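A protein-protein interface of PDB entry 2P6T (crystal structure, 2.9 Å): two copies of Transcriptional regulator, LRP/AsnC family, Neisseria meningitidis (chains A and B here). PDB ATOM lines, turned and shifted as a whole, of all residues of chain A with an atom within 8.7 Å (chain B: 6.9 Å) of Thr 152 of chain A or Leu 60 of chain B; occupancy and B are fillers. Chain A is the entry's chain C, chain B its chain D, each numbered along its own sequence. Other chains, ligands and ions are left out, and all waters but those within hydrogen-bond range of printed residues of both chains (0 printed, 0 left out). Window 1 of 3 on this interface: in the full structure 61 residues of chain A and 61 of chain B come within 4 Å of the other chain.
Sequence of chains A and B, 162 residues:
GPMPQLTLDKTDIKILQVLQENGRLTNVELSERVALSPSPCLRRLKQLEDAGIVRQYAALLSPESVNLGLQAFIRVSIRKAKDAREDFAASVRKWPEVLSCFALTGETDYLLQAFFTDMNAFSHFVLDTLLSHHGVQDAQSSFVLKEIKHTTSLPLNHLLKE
NE of Arg 55 of chain A sits at hydrogen-bond distance from O of Leu 61 of chain B.
The side-chain amino group (NZ) of Lys 149 of chain A sits at hydrogen-bond distance from the backbone carbonyl oxygen (O) of Leu 99 of chain B (3.5 Å).
The backbone carbonyl oxygen of Gln 20 of chain B lies within hydrogen-bond range of the side-chain amide nitrogen of Gln 56 of chain A (3.4 Å).
The backbone NH (N) of Ala 59 of chain B sits at hydrogen-bond distance from the backbone carbonyl oxygen (O) of Leu 19 of chain A, at 3.1 Å.
The backbone NH (N) of Ala 58 of chain A is in hydrogen-bond range of the backbone carbonyl oxygen (O) of Ala 58 of chain B.
A ring nitrogen (ND1) of His 150 of chain A sits at hydrogen-bond distance from the guanidinium group of Arg 55 of chain B (3.1 Å).
The backbone carbonyl oxygen of Gln 56 of chain A is in hydrogen-bond range of the backbone NH of Leu 60 of chain B (2.5 Å).
N of Thr 151 of chain A is in hydrogen-bond range of O of Leu 99 of chain B (3.1 Å).
The backbone NH of Arg 55 of chain A is in hydrogen-bond range of the backbone carbonyl oxygen of Leu 60 of chain B (2.9 Å).
N of Arg 55 of chain B is in hydrogen-bond range of O of Leu 60 of chain A, at 3.0 Å.
The backbone NH (N) of Ser 62 of chain B is in hydrogen-bond range of the backbone carbonyl oxygen (O) of Ile 53 of chain A (2.9 Å).
The backbone NH (N) of Leu 60 of chain A lies within hydrogen-bond range of the backbone carbonyl oxygen (O) of Gln 56 of chain B.
The backbone carbonyl oxygen of Leu 48 of chain A lies within hydrogen-bond range of the backbone NH of Val 54 of chain A (3.4 Å).
The backbone carbonyl oxygen of Leu 48 of chain A sits close to the backbone NH of Ile 53 of chain A, 3.3 Å away.
OE2 of Glu 21 of chain A sits at hydrogen-bond distance from OG of Ser 153 of chain A, 3.0 Å away.
The side-chain amide oxygen of Gln 20 of chain A sits close to the backbone NH of Leu 154 of chain A, at 3.4 Å.
The side-chain hydroxyl (OG1) of Thr 151 of chain A lies within hydrogen-bond range of the backbone NH (N) of Ser 153 of chain A (3.2 Å).
O of Gln 20 of chain A sits close to OG of Ser 153 of chain A, 3.4 Å away.
O of Ile 53 of chain A touches CD2 of Leu 61 of chain B (3.0 Å).
Ser 62 of chain B touches Arg 55 of chain A (CA to CD, 3.9 Å).
O of Gln 20 of chain B touches CB of Ala 58 of chain A, at 3.2 Å.
CG of Gln 20 of chain B touches O of Ala 59 of chain A (3.3 Å).
C of Ala 59 of chain A touches O of Gln 56 of chain B, 3.6 Å away.
O of Leu 99 of chain B touches CA of His 150 of chain A, at 3.6 Å.
His 150 of chain A touches Ser 100 of chain B.
Thr 152 of chain A touches Ala 58 of chain B (OG1 to CB, 3.8 Å).
CB of Thr 152 of chain A touches CD2 of Leu 60 of chain B (3.6 Å).
O of Ser 153 of chain A touches CG of Leu 99 of chain B, 3.6 Å away.
Of the printed residues of chain B, Arg 55 of chain A touches Leu 60, Leu 61, Ser 62 and His 150.
Of chain B, only Ala 58 (3.8 Å) and Leu 60 (3.6 Å) come within 4 Å of Thr 152 of chain A.
Of the printed residues of chain A, Gln 20 of chain B touches Gln 56, Ala 58 and Ala 59.
Of chain A, only Val 54, Arg 55, Gln 56, Ala 58 and Thr 152 come within 4 Å of Leu 60 of chain B.
Printed residues of chain A within 4 Å of Leu 99 of chain B: Lys 149 (3.5 Å), His 150 (3.6 Å), Thr 151 (3.1 Å) and Ser 153 (3.6 Å).
The nearest residue of chain B that does not touch Thr 152 of chain A is Leu 99 of chain B (4.3 Å).
Of the 24 printed residues of chain A, 19 touch a printed residue of chain B.
Hydrophobic or aromatic side chains of chain B within 4 Å of the printed part of chain A: Ala 58, Ala 59, Leu 60, Leu 61, Leu 99 and His 150.
Among the printed residues, 40 pairs touch across the chains.
Arg 55 of chain A touches Leu 60 of chain B, and with the chains exchanged Leu 60 of chain A touches Arg 55 of chain B.
Arg 55 of chain A touches His 150 of chain B, and with the chains exchanged His 150 of chain A touches Arg 55 of chain B.
Gln 56 of chain A touches Ala 59 of chain B, and with the chains exchanged Ala 59 of chain A touches Gln 56 of chain B.
Ala 58 of chain B touches its own counterpart, Ala 58 of chain A.
9 positions are printed for both chains.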
ATOM      1  N   LEU A  16       3.739  28.430  -0.592  1.00  0.00           N
ATOM      2  CA  LEU A  16       4.190  27.078  -0.249  1.00  0.00           C
ATOM      3  C   LEU A  16       4.769  26.977   1.161  1.00  0.00           C
ATOM      4  O   LEU A  16       4.523  25.996   1.866  1.00  0.00           O
ATOM      5  CB  LEU A  16       5.233  26.596  -1.258  1.00  0.00           C
ATOM      6  CG  LEU A  16       4.743  26.413  -2.699  1.00  0.00           C
ATOM      7  CD1 LEU A  16       5.929  26.205  -3.647  1.00  0.00           C
ATOM      8  CD2 LEU A  16       3.745  25.259  -2.810  1.00  0.00           C
ATOM      9  N   LEU A  19       1.778  27.114   3.519  1.00  0.00           N
ATOM     10  CA  LEU A  19       0.896  25.934   3.390  1.00  0.00           C
ATOM     11  C   LEU A  19       1.511  24.614   3.857  1.00  0.00           C
ATOM     12  O   LEU A  19       0.792  23.725   4.320  1.00  0.00           O
ATOM     13  CB  LEU A  19       0.408  25.753   1.949  1.00  0.00           C
ATOM     14  CG  LEU A  19      -0.664  26.718   1.448  1.00  0.00           C
ATOM     15  CD1 LEU A  19      -1.170  26.252   0.098  1.00  0.00           C
ATOM     16  CD2 LEU A  19      -1.812  26.828   2.436  1.00  0.00           C
ATOM     17  N   GLN A  20       2.825  24.470   3.719  1.00  0.00           N
ATOM     18  CA  GLN A  20       3.505  23.272   4.206  1.00  0.00           C
ATOM     19  C   GLN A  20       3.394  23.122   5.721  1.00  0.00           C
ATOM     20  O   GLN A  20       3.447  22.008   6.233  1.00  0.00           O
ATOM     21  CB  GLN A  20       4.975  23.274   3.796  1.00  0.00           C
ATOM     22  CG  GLN A  20       5.253  22.511   2.524  1.00  0.00           C
ATOM     23  CD  GLN A  20       6.715  22.535   2.137  1.00  0.00           C
ATOM     24  OE1 GLN A  20       7.161  21.730   1.318  1.00  0.00           O
ATOM     25  NE2 GLN A  20       7.476  23.458   2.730  1.00  0.00           N
ATOM     26  N   GLU A  21       3.235  24.240   6.426  1.00  0.00           N
ATOM     27  CA  GLU A  21       3.117  24.237   7.882  1.00  0.00           C
ATOM     28  C   GLU A  21       1.634  24.167   8.294  1.00  0.00           C
ATOM     29  O   GLU A  21       1.263  23.379   9.173  1.00  0.00           O
ATOM     30  CB  GLU A  21       3.783  25.487   8.476  1.00  0.00           C
ATOM     31  CG  GLU A  21       5.096  25.913   7.797  1.00  0.00           C
ATOM     32  CD  GLU A  21       6.339  25.530   8.572  1.00  0.00           C
ATOM     33  OE1 GLU A  21       6.649  26.207   9.576  1.00  0.00           O
ATOM     34  OE2 GLU A  21       7.024  24.572   8.156  1.00  0.00           O
ATOM     35  N   ASN A  22       0.797  24.985   7.645  1.00  0.00           N
ATOM     36  CA  ASN A  22      -0.647  25.054   7.930  1.00  0.00           C
ATOM     37  C   ASN A  22      -1.495  24.571   6.753  1.00  0.00           C
ATOM     38  O   ASN A  22      -2.263  25.326   6.173  1.00  0.00           O
ATOM     39  CB  ASN A  22      -1.064  26.485   8.290  1.00  0.00           C
ATOM     40  CG  ASN A  22      -0.211  27.086   9.387  1.00  0.00           C
ATOM     41  OD1 ASN A  22      -0.630  27.154  10.542  1.00  0.00           O
ATOM     42  ND2 ASN A  22       0.991  27.538   9.031  1.00  0.00           N
ATOM     43  N   GLY A  23      -1.377  23.293   6.426  1.00  0.00           N
ATOM     44  CA  GLY A  23      -2.056  22.728   5.266  1.00  0.00           C
ATOM     45  C   GLY A  23      -3.545  22.989   5.210  1.00  0.00           C
ATOM     46  O   GLY A  23      -4.132  22.964   4.133  1.00  0.00           O
ATOM     47  N   LEU A  48      -0.544  26.087  -8.647  1.00  0.00           N
ATOM     48  CA  LEU A  48       0.521  25.399  -7.925  1.00  0.00           C
ATOM     49  C   LEU A  48       0.186  23.924  -7.673  1.00  0.00           C
ATOM     50  O   LEU A  48       1.083  23.082  -7.683  1.00  0.00           O
ATOM     51  CB  LEU A  48       0.844  26.118  -6.604  1.00  0.00           C
ATOM     52  CG  LEU A  48       1.958  27.170  -6.653  1.00  0.00           C
ATOM     53  CD1 LEU A  48       2.120  27.872  -5.305  1.00  0.00           C
ATOM     54  CD2 LEU A  48       3.273  26.544  -7.075  1.00  0.00           C
ATOM     55  N   GLU A  49      -1.092  23.602  -7.462  1.00  0.00           N
ATOM     56  CA  GLU A  49      -1.484  22.198  -7.262  1.00  0.00           C
ATOM     57  C   GLU A  49      -1.949  21.508  -8.548  1.00  0.00           C
ATOM     58  O   GLU A  49      -1.900  20.280  -8.654  1.00  0.00           O
ATOM     59  CB  GLU A  49      -2.499  22.030  -6.116  1.00  0.00           C
ATOM     60  CG  GLU A  49      -3.807  22.799  -6.208  1.00  0.00           C
ATOM     61  CD  GLU A  49      -4.726  22.484  -5.031  1.00  0.00           C
ATOM     62  OE1 GLU A  49      -5.117  21.308  -4.880  1.00  0.00           O
ATOM     63  OE2 GLU A  49      -5.057  23.398  -4.247  1.00  0.00           O
ATOM     64  N   GLY A  52       1.584  20.208  -9.849  1.00  0.00           N
ATOM     65  CA  GLY A  52       2.194  19.094  -9.136  1.00  0.00           C
ATOM     66  C   GLY A  52       3.065  19.524  -7.969  1.00  0.00           C
ATOM     67  O   GLY A  52       3.393  18.706  -7.105  1.00  0.00           O
ATOM     68  N   ILE A  53       3.458  20.797  -7.945  1.00  0.00           N
ATOM     69  CA  ILE A  53       4.170  21.370  -6.801  1.00  0.00           C
ATOM     70  C   ILE A  53       3.598  20.842  -5.494  1.00  0.00           C
ATOM     71  O   ILE A  53       4.326  20.265  -4.688  1.00  0.00           O
ATOM     72  CB  ILE A  53       4.086  22.916  -6.767  1.00  0.00           C
ATOM     73  CG1 ILE A  53       4.909  23.531  -7.897  1.00  0.00           C
ATOM     74  CG2 ILE A  53       4.570  23.456  -5.426  1.00  0.00           C
ATOM     75  CD1 ILE A  53       4.254  23.435  -9.261  1.00  0.00           C
ATOM     76  N   VAL A  54       2.298  21.047  -5.293  1.00  0.00           N
ATOM     77  CA  VAL A  54       1.604  20.553  -4.107  1.00  0.00           C
ATOM     78  C   VAL A  54       1.022  19.184  -4.410  1.00  0.00           C
ATOM     79  O   VAL A  54      -0.074  19.079  -4.978  1.00  0.00           O
ATOM     80  CB  VAL A  54       0.475  21.504  -3.682  1.00  0.00           C
ATOM     81  CG1 VAL A  54      -0.411  20.851  -2.630  1.00  0.00           C
ATOM     82  CG2 VAL A  54       1.049  22.826  -3.173  1.00  0.00           C
ATOM     83  N   ARG A  55       1.759  18.139  -4.034  1.00  0.00           N
ATOM     84  CA  ARG A  55       1.397  16.762  -4.407  1.00  0.00           C
ATOM     85  C   ARG A  55       0.298  16.144  -3.528  1.00  0.00           C
ATOM     86  O   ARG A  55      -0.356  15.183  -3.946  1.00  0.00           O
ATOM     87  CB  ARG A  55       2.640  15.849  -4.468  1.00  0.00           C
ATOM     88  CG  ARG A  55       3.421  15.697  -3.173  1.00  0.00           C
ATOM     89  CD  ARG A  55       4.556  14.677  -3.307  1.00  0.00           C
ATOM     90  NE  ARG A  55       5.282  14.522  -2.045  1.00  0.00           N
ATOM     91  CZ  ARG A  55       4.836  13.841  -0.989  1.00  0.00           C
ATOM     92  NH1 ARG A  55       3.659  13.215  -1.023  1.00  0.00           N
ATOM     93  NH2 ARG A  55       5.578  13.778   0.117  1.00  0.00           N
ATOM     94  N   GLN A  56       0.090  16.700  -2.334  1.00  0.00           N
ATOM     95  CA  GLN A  56      -0.924  16.198  -1.399  1.00  0.00           C
ATOM     96  C   GLN A  56      -1.071  17.130  -0.181  1.00  0.00           C
ATOM     97  O   GLN A  56      -0.108  17.782   0.240  1.00  0.00           O
ATOM     98  CB  GLN A  56      -0.562  14.765  -0.955  1.00  0.00           C
ATOM     99  CG  GLN A  56      -1.431  14.158   0.145  1.00  0.00           C
ATOM    100  CD  GLN A  56      -0.901  12.822   0.672  1.00  0.00           C
ATOM    101  OE1 GLN A  56       0.018  12.230   0.103  1.00  0.00           O
ATOM    102  NE2 GLN A  56      -1.482  12.350   1.777  1.00  0.00           N
ATOM    103  N   TYR A  57      -2.287  17.207   0.355  1.00  0.00           N
ATOM    104  CA  TYR A  57      -2.545  17.815   1.658  1.00  0.00           C
ATOM    105  C   TYR A  57      -2.907  16.669   2.609  1.00  0.00           C
ATOM    106  O   TYR A  57      -3.844  15.918   2.326  1.00  0.00           O
ATOM    107  CB  TYR A  57      -3.725  18.787   1.585  1.00  0.00           C
ATOM    108  CG  TYR A  57      -3.511  20.051   0.781  1.00  0.00           C
ATOM    109  CD1 TYR A  57      -3.128  21.232   1.400  1.00  0.00           C
ATOM    110  CD2 TYR A  57      -3.734  20.075  -0.585  1.00  0.00           C
ATOM    111  CE1 TYR A  57      -2.954  22.405   0.673  1.00  0.00           C
ATOM    112  CE2 TYR A  57      -3.561  21.238  -1.323  1.00  0.00           C
ATOM    113  CZ  TYR A  57      -3.174  22.400  -0.689  1.00  0.00           C
ATOM    114  OH  TYR A  57      -3.005  23.555  -1.414  1.00  0.00           O
ATOM    115  N   ALA A  58      -2.184  16.531   3.726  1.00  0.00           N
ATOM    116  CA  ALA A  58      -2.400  15.400   4.656  1.00  0.00           C
ATOM    117  C   ALA A  58      -2.381  15.785   6.138  1.00  0.00           C
ATOM    118  O   ALA A  58      -1.723  16.750   6.538  1.00  0.00           O
ATOM    119  CB  ALA A  58      -1.374  14.298   4.398  1.00  0.00           C
ATOM    120  N   ALA A  59      -3.110  15.007   6.936  1.00  0.00           N
ATOM    121  CA  ALA A  59      -3.133  15.163   8.381  1.00  0.00           C
ATOM    122  C   ALA A  59      -2.043  14.282   8.934  1.00  0.00           C
ATOM    123  O   ALA A  59      -1.987  13.089   8.628  1.00  0.00           O
ATOM    124  CB  ALA A  59      -4.472  14.743   8.942  1.00  0.00           C
ATOM    125  N   LEU A  60      -1.165  14.868   9.735  1.00  0.00           N
ATOM    126  CA  LEU A  60      -0.083  14.115  10.341  1.00  0.00           C
ATOM    127  C   LEU A  60      -0.462  13.753  11.766  1.00  0.00           C
ATOM    128  O   LEU A  60      -0.781  14.623  12.568  1.00  0.00           O
ATOM    129  CB  LEU A  60       1.209  14.928  10.313  1.00  0.00           C
ATOM    130  CG  LEU A  60       1.687  15.342   8.918  1.00  0.00           C
ATOM    131  CD1 LEU A  60       3.132  15.823   8.961  1.00  0.00           C
ATOM    132  CD2 LEU A  60       1.547  14.198   7.925  1.00  0.00           C
ATOM    133  N   LYS A 149      14.244  15.747  15.626  1.00  0.00           N
ATOM    134  CA  LYS A 149      13.558  16.630  14.687  1.00  0.00           C
ATOM    135  C   LYS A 149      12.825  15.835  13.610  1.00  0.00           C
ATOM    136  O   LYS A 149      13.339  14.837  13.106  1.00  0.00           O
ATOM    137  CB  LYS A 149      14.578  17.587  14.052  1.00  0.00           C
ATOM    138  CG  LYS A 149      13.996  18.708  13.188  1.00  0.00           C
ATOM    139  CD  LYS A 149      15.090  19.357  12.321  1.00  0.00           C
ATOM    140  CE  LYS A 149      14.650  20.700  11.743  1.00  0.00           C
ATOM    141  NZ  LYS A 149      13.527  20.569  10.776  1.00  0.00           N
ATOM    142  N   HIS A 150      11.619  16.272  13.267  1.00  0.00           N
ATOM    143  CA  HIS A 150      10.884  15.672  12.161  1.00  0.00           C
ATOM    144  C   HIS A 150       9.855  16.649  11.610  1.00  0.00           C
ATOM    145  O   HIS A 150       8.875  16.971  12.285  1.00  0.00           O
ATOM    146  CB  HIS A 150      10.200  14.376  12.596  1.00  0.00           C
ATOM    147  CG  HIS A 150       9.420  13.715  11.504  1.00  0.00           C
ATOM    148  ND1 HIS A 150       8.055  13.855  11.375  1.00  0.00           N
ATOM    149  CD2 HIS A 150       9.814  12.924  10.481  1.00  0.00           C
ATOM    150  CE1 HIS A 150       7.639  13.172  10.322  1.00  0.00           C
ATOM    151  NE2 HIS A 150       8.688  12.601   9.760  1.00  0.00           N
ATOM    152  N   THR A 151      10.098  17.117  10.386  1.00  0.00           N
ATOM    153  CA  THR A 151       9.176  18.001   9.674  1.00  0.00           C
ATOM    154  C   THR A 151       8.954  17.502   8.256  1.00  0.00           C
ATOM    155  O   THR A 151       9.872  16.972   7.634  1.00  0.00           O
ATOM    156  CB  THR A 151       9.715  19.442   9.583  1.00  0.00           C
ATOM    157  OG1 THR A 151       8.726  20.277   8.976  1.00  0.00           O
ATOM    158  CG2 THR A 151      10.979  19.507   8.745  1.00  0.00           C
ATOM    159  N   THR A 152       7.743  17.684   7.739  1.00  0.00           N
ATOM    160  CA  THR A 152       7.454  17.350   6.341  1.00  0.00           C
ATOM    161  C   THR A 152       7.802  18.502   5.376  1.00  0.00           C
ATOM    162  O   THR A 152       7.765  18.321   4.158  1.00  0.00           O
ATOM    163  CB  THR A 152       5.972  16.936   6.143  1.00  0.00           C
ATOM    164  OG1 THR A 152       5.117  17.870   6.816  1.00  0.00           O
ATOM    165  CG2 THR A 152       5.720  15.532   6.688  1.00  0.00           C
ATOM    166  N   SER A 153       8.154  19.670   5.918  1.00  0.00           N
ATOM    167  CA  SER A 153       8.420  20.865   5.102  1.00  0.00           C
ATOM    168  C   SER A 153       9.845  20.908   4.531  1.00  0.00           C
ATOM    169  O   SER A 153      10.829  20.837   5.271  1.00  0.00           O
ATOM    170  CB  SER A 153       8.155  22.139   5.913  1.00  0.00           C
ATOM    171  OG  SER A 153       6.810  22.200   6.358  1.00  0.00           O
ATOM    172  N   LEU A 154       9.925  21.051   3.209  1.00  0.00           N
ATOM    173  CA  LEU A 154      11.189  21.154   2.471  1.00  0.00           C
ATOM    174  C   LEU A 154      11.708  22.593   2.587  1.00  0.00           C
ATOM    175  O   LEU A 154      10.923  23.511   2.844  1.00  0.00           O
ATOM    176  CB  LEU A 154      10.980  20.823   0.979  1.00  0.00           C
ATOM    177  CG  LEU A 154      10.344  19.508   0.483  1.00  0.00           C
ATOM    178  CD1 LEU A 154       8.872  19.320   0.874  1.00  0.00           C
ATOM    179  CD2 LEU A 154      10.457  19.456  -1.038  1.00  0.00           C
ATOM    180  N   PRO A 155      13.028  22.800   2.391  1.00  0.00           N
ATOM    181  CA  PRO A 155      13.582  24.156   2.333  1.00  0.00           C
ATOM    182  C   PRO A 155      13.307  24.764   0.972  1.00  0.00           C
ATOM    183  O   PRO A 155      13.305  24.041  -0.022  1.00  0.00           O
ATOM    184  CB  PRO A 155      15.080  23.921   2.506  1.00  0.00           C
ATOM    185  CG  PRO A 155      15.301  22.607   1.859  1.00  0.00           C
ATOM    186  CD  PRO A 155      14.081  21.784   2.209  1.00  0.00           C
ATOM    187  N   GLN B  20      -5.780  11.469   6.997  1.00  0.00           N
ATOM    188  CA  GLN B  20      -4.354  11.310   6.705  1.00  0.00           C
ATOM    189  C   GLN B  20      -4.069  11.315   5.209  1.00  0.00           C
ATOM    190  O   GLN B  20      -2.933  11.540   4.800  1.00  0.00           O
ATOM    191  CB  GLN B  20      -3.824  10.011   7.311  1.00  0.00           C
ATOM    192  CG  GLN B  20      -3.437  10.137   8.776  1.00  0.00           C
ATOM    193  CD  GLN B  20      -2.967   8.832   9.378  1.00  0.00           C
ATOM    194  OE1 GLN B  20      -2.222   8.825  10.355  1.00  0.00           O
ATOM    195  NE2 GLN B  20      -3.396   7.716   8.793  1.00  0.00           N
ATOM    196  N   ARG B  55      -1.551  15.921  15.169  1.00  0.00           N
ATOM    197  CA  ARG B  55      -0.564  16.919  15.571  1.00  0.00           C
ATOM    198  C   ARG B  55      -0.567  18.130  14.634  1.00  0.00           C
ATOM    199  O   ARG B  55      -0.398  19.262  15.094  1.00  0.00           O
ATOM    200  CB  ARG B  55       0.843  16.301  15.682  1.00  0.00           C
ATOM    201  CG  ARG B  55       1.417  15.742  14.384  1.00  0.00           C
ATOM    202  CD  ARG B  55       2.886  15.371  14.503  1.00  0.00           C
ATOM    203  NE  ARG B  55       3.556  15.460  13.205  1.00  0.00           N
ATOM    204  CZ  ARG B  55       4.727  14.902  12.904  1.00  0.00           C
ATOM    205  NH1 ARG B  55       5.401  14.182  13.800  1.00  0.00           N
ATOM    206  NH2 ARG B  55       5.220  15.062  11.683  1.00  0.00           N
ATOM    207  N   GLN B  56      -0.762  17.901  13.334  1.00  0.00           N
ATOM    208  CA  GLN B  56      -0.852  19.003  12.364  1.00  0.00           C
ATOM    209  C   GLN B  56      -1.379  18.590  10.986  1.00  0.00           C
ATOM    210  O   GLN B  56      -1.339  17.415  10.592  1.00  0.00           O
ATOM    211  CB  GLN B  56       0.501  19.717  12.195  1.00  0.00           C
ATOM    212  CG  GLN B  56       1.661  18.803  11.819  1.00  0.00           C
ATOM    213  CD  GLN B  56       2.895  19.574  11.384  1.00  0.00           C
ATOM    214  OE1 GLN B  56       2.834  20.389  10.463  1.00  0.00           O
ATOM    215  NE2 GLN B  56       4.028  19.311  12.038  1.00  0.00           N
ATOM    216  N   ALA B  58      -0.658  19.475   7.123  1.00  0.00           N
ATOM    217  CA  ALA B  58       0.380  20.067   6.266  1.00  0.00           C
ATOM    218  C   ALA B  58       0.201  19.753   4.769  1.00  0.00           C
ATOM    219  O   ALA B  58      -0.353  18.714   4.388  1.00  0.00           O
ATOM    220  CB  ALA B  58       1.761  19.623   6.738  1.00  0.00           C
ATOM    221  N   ALA B  59       0.673  20.683   3.938  1.00  0.00           N
ATOM    222  CA  ALA B  59       0.698  20.520   2.492  1.00  0.00           C
ATOM    223  C   ALA B  59       2.003  19.835   2.122  1.00  0.00           C
ATOM    224  O   ALA B  59       3.076  20.311   2.477  1.00  0.00           O
ATOM    225  CB  ALA B  59       0.600  21.878   1.811  1.00  0.00           C
ATOM    226  N   LEU B  60       1.914  18.717   1.416  1.00  0.00           N
ATOM    227  CA  LEU B  60       3.099  17.953   1.051  1.00  0.00           C
ATOM    228  C   LEU B  60       3.504  18.288  -0.366  1.00  0.00           C
ATOM    229  O   LEU B  60       2.733  18.046  -1.297  1.00  0.00           O
ATOM    230  CB  LEU B  60       2.817  16.460   1.170  1.00  0.00           C
ATOM    231  CG  LEU B  60       2.432  16.004   2.579  1.00  0.00           C
ATOM    232  CD1 LEU B  60       2.097  14.528   2.565  1.00  0.00           C
ATOM    233  CD2 LEU B  60       3.541  16.308   3.600  1.00  0.00           C
ATOM    234  N   LEU B  61       4.707  18.841  -0.524  1.00  0.00           N
ATOM    235  CA  LEU B  61       5.200  19.247  -1.841  1.00  0.00           C
ATOM    236  C   LEU B  61       6.097  18.197  -2.510  1.00  0.00           C
ATOM    237  O   LEU B  61       6.580  17.269  -1.861  1.00  0.00           O
ATOM    238  CB  LEU B  61       5.960  20.559  -1.729  1.00  0.00           C
ATOM    239  CG  LEU B  61       5.166  21.791  -1.314  1.00  0.00           C
ATOM    240  CD1 LEU B  61       6.137  22.954  -1.113  1.00  0.00           C
ATOM    241  CD2 LEU B  61       4.125  22.142  -2.353  1.00  0.00           C
ATOM    242  N   SER B  62       6.316  18.368  -3.813  1.00  0.00           N
ATOM    243  CA  SER B  62       7.056  17.402  -4.637  1.00  0.00           C
ATOM    244  C   SER B  62       8.517  17.855  -4.802  1.00  0.00           C
ATOM    245  O   SER B  62       8.777  18.874  -5.430  1.00  0.00           O
ATOM    246  CB  SER B  62       6.362  17.242  -6.004  1.00  0.00           C
ATOM    247  OG  SER B  62       7.007  16.283  -6.827  1.00  0.00           O
ATOM    248  N   LEU B  99      15.253  17.788   7.215  1.00  0.00           N
ATOM    249  CA  LEU B  99      13.855  17.550   7.603  1.00  0.00           C
ATOM    250  C   LEU B  99      13.748  16.765   8.918  1.00  0.00           C
ATOM    251  O   LEU B  99      13.112  17.229   9.873  1.00  0.00           O
ATOM    252  CB  LEU B  99      13.091  16.808   6.504  1.00  0.00           C
ATOM    253  CG  LEU B  99      12.540  17.670   5.376  1.00  0.00           C
ATOM    254  CD1 LEU B  99      13.652  18.467   4.721  1.00  0.00           C
ATOM    255  CD2 LEU B  99      11.817  16.790   4.361  1.00  0.00           C
ATOM    256  N   SER B 100      14.367  15.582   8.954  1.00  0.00           N
ATOM    257  CA  SER B 100      14.283  14.686  10.113  1.00  0.00           C
ATOM    258  C   SER B 100      15.633  14.495  10.802  1.00  0.00           C
ATOM    259  O   SER B 100      16.683  14.617  10.176  1.00  0.00           O
ATOM    260  CB  SER B 100      13.749  13.314   9.692  1.00  0.00           C
ATOM    261  OG  SER B 100      12.559  13.423   8.934  1.00  0.00           O
ATOM    262  N   HIS B 150       6.555   6.152  -0.275  1.00  0.00           N
ATOM    263  CA  HIS B 150       6.620   7.222   0.703  1.00  0.00           C
ATOM    264  C   HIS B 150       5.228   7.771   0.964  1.00  0.00           C
ATOM    265  O   HIS B 150       4.603   8.356   0.075  1.00  0.00           O
ATOM    266  CB  HIS B 150       7.533   8.356   0.241  1.00  0.00           C
ATOM    267  CG  HIS B 150       7.685   9.449   1.254  1.00  0.00           C
ATOM    268  ND1 HIS B 150       6.777  10.481   1.374  1.00  0.00           N
ATOM    269  CD2 HIS B 150       8.622   9.660   2.209  1.00  0.00           C
ATOM    270  CE1 HIS B 150       7.158  11.288   2.347  1.00  0.00           C
ATOM    271  NE2 HIS B 150       8.275  10.813   2.871  1.00  0.00           N
ATOM    272  N   THR B 151       4.760   7.568   2.190  1.00  0.00           N
ATOM    273  CA  THR B 151       3.475   8.075   2.648  1.00  0.00           C
ATOM    274  C   THR B 151       3.651   8.572   4.088  1.00  0.00           C
ATOM    275  O   THR B 151       4.475   8.051   4.838  1.00  0.00           O
ATOM    276  CB  THR B 151       2.338   6.973   2.517  1.00  0.00           C
ATOM    277  OG1 THR B 151       1.121   7.398   3.162  1.00  0.00           O
ATOM    278  CG2 THR B 151       2.780   5.654   3.113  1.00  0.00           C
ATOM    279  N   THR B 152       2.883   9.591   4.455  1.00  0.00           N
ATOM    280  CA  THR B 152       2.860  10.093   5.827  1.00  0.00           C
ATOM    281  C   THR B 152       1.847   9.333   6.682  1.00  0.00           C
ATOM    282  O   THR B 152       1.818   9.479   7.897  1.00  0.00           O
ATOM    283  CB  THR B 152       2.476  11.577   5.874  1.00  0.00           C
ATOM    284  OG1 THR B 152       1.046  11.703   5.920  1.00  0.00           O
ATOM    285  CG2 THR B 152       3.035  12.326   4.665  1.00  0.00           C
